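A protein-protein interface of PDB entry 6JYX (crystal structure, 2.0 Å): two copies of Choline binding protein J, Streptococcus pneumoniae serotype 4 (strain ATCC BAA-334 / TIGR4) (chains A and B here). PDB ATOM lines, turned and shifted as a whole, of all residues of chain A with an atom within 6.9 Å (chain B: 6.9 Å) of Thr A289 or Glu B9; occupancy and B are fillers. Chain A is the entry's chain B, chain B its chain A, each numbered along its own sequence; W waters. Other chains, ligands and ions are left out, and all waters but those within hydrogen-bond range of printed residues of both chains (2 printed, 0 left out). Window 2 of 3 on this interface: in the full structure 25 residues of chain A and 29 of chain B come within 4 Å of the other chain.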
ATOM      1  N   TYR A 279      -7.238  -4.446   2.756  1.00  0.00           N
ATOM      2  CA  TYR A 279      -6.392  -5.366   2.031  1.00  0.00           C
ATOM      3  C   TYR A 279      -6.298  -4.926   0.544  1.00  0.00           C
ATOM      4  O   TYR A 279      -7.003  -3.994   0.110  1.00  0.00           O
ATOM      5  CB  TYR A 279      -7.007  -6.775   2.103  1.00  0.00           C
ATOM      6  CG  TYR A 279      -7.191  -7.287   3.514  1.00  0.00           C
ATOM      7  CD1 TYR A 279      -8.469  -7.425   4.072  1.00  0.00           C
ATOM      8  CD2 TYR A 279      -6.087  -7.611   4.305  1.00  0.00           C
ATOM      9  CE1 TYR A 279      -8.639  -7.873   5.392  1.00  0.00           C
ATOM     10  CE2 TYR A 279      -6.250  -8.033   5.622  1.00  0.00           C
ATOM     11  CZ  TYR A 279      -7.520  -8.169   6.151  1.00  0.00           C
ATOM     12  OH  TYR A 279      -7.692  -8.611   7.440  1.00  0.00           O
ATOM     13  N   ALA A 285     -10.175  -4.478   6.853  1.00  0.00           N
ATOM     14  CA  ALA A 285      -9.743  -5.467   7.871  1.00  0.00           C
ATOM     15  C   ALA A 285     -10.442  -5.151   9.178  1.00  0.00           C
ATOM     16  O   ALA A 285     -10.501  -3.966   9.593  1.00  0.00           O
ATOM     17  CB  ALA A 285      -8.245  -5.383   8.048  1.00  0.00           C
ATOM     18  N   VAL A 286     -10.986  -6.185   9.833  1.00  0.00           N
ATOM     19  CA  VAL A 286     -11.679  -5.996  11.119  1.00  0.00           C
ATOM     20  C   VAL A 286     -11.277  -7.061  12.164  1.00  0.00           C
ATOM     21  O   VAL A 286     -10.965  -8.198  11.799  1.00  0.00           O
ATOM     22  CB  VAL A 286     -13.259  -6.024  10.974  1.00  0.00           C
ATOM     23  CG1 VAL A 286     -13.744  -4.906   9.999  1.00  0.00           C
ATOM     24  CG2 VAL A 286     -13.746  -7.402  10.499  1.00  0.00           C
ATOM     25  N   ASN A 287     -11.311  -6.688  13.447  1.00  0.00           N
ATOM     26  CA  ASN A 287     -11.106  -7.678  14.549  1.00  0.00           C
ATOM     27  C   ASN A 287      -9.869  -8.534  14.314  1.00  0.00           C
ATOM     28  O   ASN A 287      -9.938  -9.771  14.336  1.00  0.00           O
ATOM     29  CB  ASN A 287     -12.301  -8.628  14.637  1.00  0.00           C
ATOM     30  CG  ASN A 287     -13.540  -7.970  15.135  1.00  0.00           C
ATOM     31  OD1 ASN A 287     -13.512  -7.142  16.065  1.00  0.00           O
ATOM     32  ND2 ASN A 287     -14.675  -8.341  14.530  1.00  0.00           N
ATOM     33  N   THR A 288      -8.745  -7.882  14.062  1.00  0.00           N
ATOM     34  CA  THR A 288      -7.551  -8.603  13.710  1.00  0.00           C
ATOM     35  C   THR A 288      -6.311  -7.754  13.939  1.00  0.00           C
ATOM     36  O   THR A 288      -6.395  -6.611  14.395  1.00  0.00           O
ATOM     37  CB  THR A 288      -7.635  -9.189  12.254  1.00  0.00           C
ATOM     38  OG1 THR A 288      -6.703 -10.258  12.141  1.00  0.00           O
ATOM     39  CG2 THR A 288      -7.356  -8.127  11.143  1.00  0.00           C
ATOM     40  N   THR A 289      -5.164  -8.344  13.646  1.00  0.00           N
ATOM     41  CA  THR A 289      -3.901  -7.616  13.638  1.00  0.00           C
ATOM     42  C   THR A 289      -3.444  -7.506  12.178  1.00  0.00           C
ATOM     43  O   THR A 289      -3.507  -8.481  11.400  1.00  0.00           O
ATOM     44  CB  THR A 289      -2.824  -8.318  14.526  1.00  0.00           C
ATOM     45  OG1 THR A 289      -3.283  -8.322  15.893  1.00  0.00           O
ATOM     46  CG2 THR A 289      -1.480  -7.542  14.489  1.00  0.00           C
ATOM     47  N   VAL A 290      -2.989  -6.311  11.831  1.00  0.00           N
ATOM     48  CA  VAL A 290      -2.464  -6.006  10.501  1.00  0.00           C
ATOM     49  C   VAL A 290      -1.106  -5.329  10.643  1.00  0.00           C
ATOM     50  O   VAL A 290      -0.997  -4.249  11.254  1.00  0.00           O
ATOM     51  CB  VAL A 290      -3.437  -5.098   9.694  1.00  0.00           C
ATOM     52  CG1 VAL A 290      -2.765  -4.667   8.400  1.00  0.00           C
ATOM     53  CG2 VAL A 290      -4.741  -5.866   9.372  1.00  0.00           C
ATOM     54  N   ASP A 291      -0.072  -5.957  10.080  1.00  0.00           N
ATOM     55  CA  ASP A 291       1.311  -5.449  10.186  1.00  0.00           C
ATOM     56  C   ASP A 291       1.671  -5.073  11.634  1.00  0.00           C
ATOM     57  O   ASP A 291       2.301  -4.040  11.861  1.00  0.00           O
ATOM     58  CB  ASP A 291       1.515  -4.206   9.294  1.00  0.00           C
ATOM     59  CG  ASP A 291       1.209  -4.465   7.813  1.00  0.00           C
ATOM     60  OD1 ASP A 291       1.184  -5.643   7.388  1.00  0.00           O
ATOM     61  OD2 ASP A 291       0.992  -3.473   7.073  1.00  0.00           O
ATOM     62  N   GLY A 292       1.214  -5.861  12.611  1.00  0.00           N
ATOM     63  CA  GLY A 292       1.487  -5.568  14.021  1.00  0.00           C
ATOM     64  C   GLY A 292       0.538  -4.603  14.716  1.00  0.00           C
ATOM     65  O   GLY A 292       0.676  -4.355  15.915  1.00  0.00           O
ATOM     66  N   TYR A 293      -0.447  -4.069  13.996  1.00  0.00           N
ATOM     67  CA  TYR A 293      -1.400  -3.133  14.588  1.00  0.00           C
ATOM     68  C   TYR A 293      -2.744  -3.793  14.842  1.00  0.00           C
ATOM     69  O   TYR A 293      -3.204  -4.599  14.020  1.00  0.00           O
ATOM     70  CB  TYR A 293      -1.597  -1.933  13.663  1.00  0.00           C
ATOM     71  CG  TYR A 293      -0.320  -1.185  13.421  1.00  0.00           C
ATOM     72  CD1 TYR A 293       0.469  -1.462  12.300  1.00  0.00           C
ATOM     73  CD2 TYR A 293       0.119  -0.212  14.320  1.00  0.00           C
ATOM     74  CE1 TYR A 293       1.657  -0.790  12.075  1.00  0.00           C
ATOM     75  CE2 TYR A 293       1.310   0.479  14.093  1.00  0.00           C
ATOM     76  CZ  TYR A 293       2.068   0.182  12.970  1.00  0.00           C
ATOM     77  OH  TYR A 293       3.238   0.857  12.738  1.00  0.00           O
ATOM     78  N   SER A 294      -3.386  -3.462  15.959  1.00  0.00           N
ATOM     79  CA  SER A 294      -4.691  -4.033  16.255  1.00  0.00           C
ATOM     80  C   SER A 294      -5.811  -3.194  15.669  1.00  0.00           C
ATOM     81  O   SER A 294      -5.833  -1.999  15.856  1.00  0.00           O
ATOM     82  CB  SER A 294      -4.920  -4.116  17.768  1.00  0.00           C
ATOM     83  OG  SER A 294      -3.930  -4.956  18.311  1.00  0.00           O
ATOM     84  N   VAL A 295      -6.761  -3.831  15.005  1.00  0.00           N
ATOM     85  CA  VAL A 295      -7.962  -3.099  14.565  1.00  0.00           C
ATOM     86  C   VAL A 295      -9.214  -3.717  15.181  1.00  0.00           C
ATOM     87  O   VAL A 295      -9.291  -4.948  15.298  1.00  0.00           O
ATOM     88  CB  VAL A 295      -8.049  -3.005  13.016  1.00  0.00           C
ATOM     89  CG1 VAL A 295      -6.805  -2.284  12.454  1.00  0.00           C
ATOM     90  CG2 VAL A 295      -8.170  -4.398  12.370  1.00  0.00           C
ATOM     91  N   VAL B   7       4.073 -16.942   5.684  1.00  0.00           N
ATOM     92  CA  VAL B   7       3.221 -16.668   6.838  1.00  0.00           C
ATOM     93  C   VAL B   7       1.790 -16.483   6.354  1.00  0.00           C
ATOM     94  O   VAL B   7       1.540 -15.716   5.414  1.00  0.00           O
ATOM     95  CB  VAL B   7       3.682 -15.398   7.575  1.00  0.00           C
ATOM     96  CG1 VAL B   7       2.888 -15.190   8.854  1.00  0.00           C
ATOM     97  CG2 VAL B   7       5.180 -15.465   7.876  1.00  0.00           C
ATOM     98  N   GLN B   8       0.868 -17.203   6.979  1.00  0.00           N
ATOM     99  CA  GLN B   8      -0.546 -17.072   6.694  1.00  0.00           C
ATOM    100  C   GLN B   8      -1.142 -16.074   7.678  1.00  0.00           C
ATOM    101  O   GLN B   8      -1.055 -16.259   8.895  1.00  0.00           O
ATOM    102  CB  GLN B   8      -1.253 -18.423   6.833  1.00  0.00           C
ATOM    103  CG  GLN B   8      -2.503 -18.563   5.978  1.00  0.00           C
ATOM    104  CD  GLN B   8      -2.192 -18.642   4.490  1.00  0.00           C
ATOM    105  OE1 GLN B   8      -1.088 -19.021   4.090  1.00  0.00           O
ATOM    106  NE2 GLN B   8      -3.166 -18.274   3.665  1.00  0.00           N
ATOM    107  N   GLU B   9      -1.741 -15.009   7.158  1.00  0.00           N
ATOM    108  CA  GLU B   9      -2.279 -13.969   8.016  1.00  0.00           C
ATOM    109  C   GLU B   9      -3.525 -13.395   7.341  1.00  0.00           C
ATOM    110  O   GLU B   9      -3.487 -13.021   6.173  1.00  0.00           O
ATOM    111  CB  GLU B   9      -1.188 -12.915   8.207  1.00  0.00           C
ATOM    112  CG  GLU B   9      -1.468 -11.846   9.200  1.00  0.00           C
ATOM    113  CD  GLU B   9      -0.187 -11.079   9.583  1.00  0.00           C
ATOM    114  OE1 GLU B   9       0.937 -11.590   9.331  1.00  0.00           O
ATOM    115  OE2 GLU B   9      -0.308  -9.967  10.134  1.00  0.00           O
ATOM    116  N   ASN B  10      -4.632 -13.381   8.070  1.00  0.00           N
ATOM    117  CA  ASN B  10      -5.889 -12.829   7.575  1.00  0.00           C
ATOM    118  C   ASN B  10      -6.304 -13.454   6.257  1.00  0.00           C
ATOM    119  O   ASN B  10      -6.785 -12.763   5.384  1.00  0.00           O
ATOM    120  CB  ASN B  10      -5.767 -11.312   7.448  1.00  0.00           C
ATOM    121  CG  ASN B  10      -5.551 -10.656   8.780  1.00  0.00           C
ATOM    122  OD1 ASN B  10      -6.319 -10.892   9.698  1.00  0.00           O
ATOM    123  ND2 ASN B  10      -4.508  -9.833   8.903  1.00  0.00           N
ATOM    124  N   GLY B  11      -6.081 -14.759   6.122  1.00  0.00           N
ATOM    125  CA  GLY B  11      -6.412 -15.484   4.886  1.00  0.00           C
ATOM    126  C   GLY B  11      -5.387 -15.315   3.755  1.00  0.00           C
ATOM    127  O   GLY B  11      -5.415 -16.063   2.772  1.00  0.00           O
ATOM    128  N   ARG B  12      -4.464 -14.364   3.903  1.00  0.00           N
ATOM    129  CA  ARG B  12      -3.468 -14.074   2.869  1.00  0.00           C
ATOM    130  C   ARG B  12      -2.136 -14.739   3.181  1.00  0.00           C
ATOM    131  O   ARG B  12      -1.886 -15.155   4.322  1.00  0.00           O
ATOM    132  CB  ARG B  12      -3.247 -12.563   2.750  1.00  0.00           C
ATOM    133  CG  ARG B  12      -4.506 -11.675   2.698  1.00  0.00           C
ATOM    134  CD  ARG B  12      -5.391 -12.023   1.526  1.00  0.00           C
ATOM    135  NE  ARG B  12      -6.306 -10.938   1.140  1.00  0.00           N
ATOM    136  CZ  ARG B  12      -7.373 -10.527   1.829  1.00  0.00           C
ATOM    137  NH1 ARG B  12      -8.124  -9.553   1.334  1.00  0.00           N
ATOM    138  NH2 ARG B  12      -7.700 -11.069   3.000  1.00  0.00           N
ATOM    139  N   THR B  13      -1.271 -14.817   2.178  1.00  0.00           N
ATOM    140  CA  THR B  13       0.073 -15.310   2.371  1.00  0.00           C
ATOM    141  C   THR B  13       1.105 -14.216   2.101  1.00  0.00           C
ATOM    142  O   THR B  13       1.025 -13.468   1.106  1.00  0.00           O
ATOM    143  CB  THR B  13       0.350 -16.582   1.523  1.00  0.00           C
ATOM    144  OG1 THR B  13      -0.598 -17.601   1.868  1.00  0.00           O
ATOM    145  CG2 THR B  13       1.729 -17.114   1.793  1.00  0.00           C
ATOM    146  N   TYR B  14       2.070 -14.129   3.011  1.00  0.00           N
ATOM    147  CA  TYR B  14       3.140 -13.141   2.974  1.00  0.00           C
ATOM    148  C   TYR B  14       4.477 -13.857   3.113  1.00  0.00           C
ATOM    149  O   TYR B  14       4.533 -14.975   3.619  1.00  0.00           O
ATOM    150  CB  TYR B  14       2.982 -12.168   4.142  1.00  0.00           C
ATOM    151  CG  TYR B  14       1.627 -11.491   4.193  1.00  0.00           C
ATOM    152  CD1 TYR B  14       0.544 -12.107   4.830  1.00  0.00           C
ATOM    153  CD2 TYR B  14       1.429 -10.237   3.601  1.00  0.00           C
ATOM    154  CE1 TYR B  14      -0.708 -11.497   4.866  1.00  0.00           C
ATOM    155  CE2 TYR B  14       0.172  -9.606   3.646  1.00  0.00           C
ATOM    156  CZ  TYR B  14      -0.886 -10.257   4.257  1.00  0.00           C
ATOM    157  OH  TYR B  14      -2.114  -9.680   4.315  1.00  0.00           O
ATOM    158  N   LYS B  16       7.728 -13.223   5.106  1.00  0.00           N
ATOM    159  CA  LYS B  16       8.225 -12.361   6.183  1.00  0.00           C
ATOM    160  C   LYS B  16       9.448 -12.943   6.894  1.00  0.00           C
ATOM    161  O   LYS B  16       9.599 -14.172   7.015  1.00  0.00           O
ATOM    162  CB  LYS B  16       7.137 -12.094   7.245  1.00  0.00           C
ATOM    163  CG  LYS B  16       5.825 -11.480   6.761  1.00  0.00           C
ATOM    164  CD  LYS B  16       5.055 -10.824   7.925  1.00  0.00           C
ATOM    165  CE  LYS B  16       3.707 -10.266   7.448  1.00  0.00           C
ATOM    166  NZ  LYS B  16       3.146  -9.139   8.261  1.00  0.00           N
ATOM    167  N   GLU B  41       0.954  -9.079  -0.184  1.00  0.00           N
ATOM    168  CA  GLU B  41       0.098 -10.251  -0.391  1.00  0.00           C
ATOM    169  C   GLU B  41       0.585 -11.002  -1.614  1.00  0.00           C
ATOM    170  O   GLU B  41       0.825 -10.397  -2.665  1.00  0.00           O
ATOM    171  CB  GLU B  41      -1.377  -9.860  -0.571  1.00  0.00           C
ATOM    172  CG  GLU B  41      -2.027  -9.194   0.670  1.00  0.00           C
ATOM    173  CD  GLU B  41      -3.434  -8.612   0.405  1.00  0.00           C
ATOM    174  OE1 GLU B  41      -4.225  -9.184  -0.389  1.00  0.00           O
ATOM    175  OE2 GLU B  41      -3.763  -7.590   1.023  1.00  0.00           O
HETATM  176  O   HOH W   1      -0.601  -8.274   8.154  1.00  0.00           O
HETATM  177  O   HOH W   2      -8.362 -12.477  10.749  1.00  0.00           O
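No position is printed for both chains. Of the 6 pairs that touch across the chains among the printed residues, none has its exchanged pair printed and touching as well.
The side-chain amide nitrogen of Gln B8 lies close to the backbone carbonyl oxygen of Arg B12 (3.4 Å). OE1 of Glu B9 is in salt-bridge range of NZ of Lys B16 (3.5 Å). The backbone carbonyl oxygen of Asn B10 sits at hydrogen-bond distance from the guanidinium group of Arg B12, 3.1 Å away. The guanidinium group (NE) of Arg B12 is in salt-bridge range of the side-chain carboxylate (OE1) of Glu B41, 3.1 Å away. The backbone carbonyl oxygen (O) of Thr A288 sits at hydrogen-bond distance from the backbone NH (N) of Val A295 (2.9 Å).
OD1 of Asn B10 sits close to OH of Tyr A279. The side-chain hydroxyl (OG1) of Thr A288 lies within hydrogen-bond range of the side-chain amide oxygen (OD1) of Asn B10, at 2.6 Å. The side-chain amide nitrogen of Asn B10 is in hydrogen-bond range of the backbone carbonyl oxygen of Thr A289, 3.0 Å away.
Of the printed residues of chain A, Glu B9 touches Thr A289 (3.7 Å). Of the printed residues of chain A, Asn B10 touches Tyr A279, Thr A288 and Thr A289. Printed residues of chain B within 4 Å of Thr A288: Asn B10. Of the printed residues of chain A, Glu B41 touches Tyr A279. Of the printed residues of chain B, Tyr A279 touches Asn B10, Arg B12 and Glu B41. Gln B8 touches none of the printed residues of chain A. Gly A292 touches none of the printed residues of chain B.
Water W1 lies within hydrogen-bond range of the side-chain carboxylate of Glu B9 (2.6 Å) and the backbone NH of Asp A291 (3.1 Å). Water W2 lies within hydrogen-bond range of the side-chain amide oxygen (OD1) of Asn B10 and the side-chain hydroxyl (OG1) of Thr A288.
Of the 10 printed residues of chain B, 4 touch a printed residue of chain A. Printed residues of chain B that touch a printed residue of chain A: Glu B9, Asn B10, Arg B12 and Glu B41. Hydrophobic or aromatic side chains of chain A within 4 Å of the printed part of chain B: Tyr A279. Among the printed residues, 6 pairs touch across the chains.
CB of Tyr A279 touches NH1 of Arg B12 (3.1 Å). CB of Tyr A279 touches OE2 of Glu B41, at 3.5 Å. Thr A289 touches Glu B9 (O to OE2, 3.7 Å).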
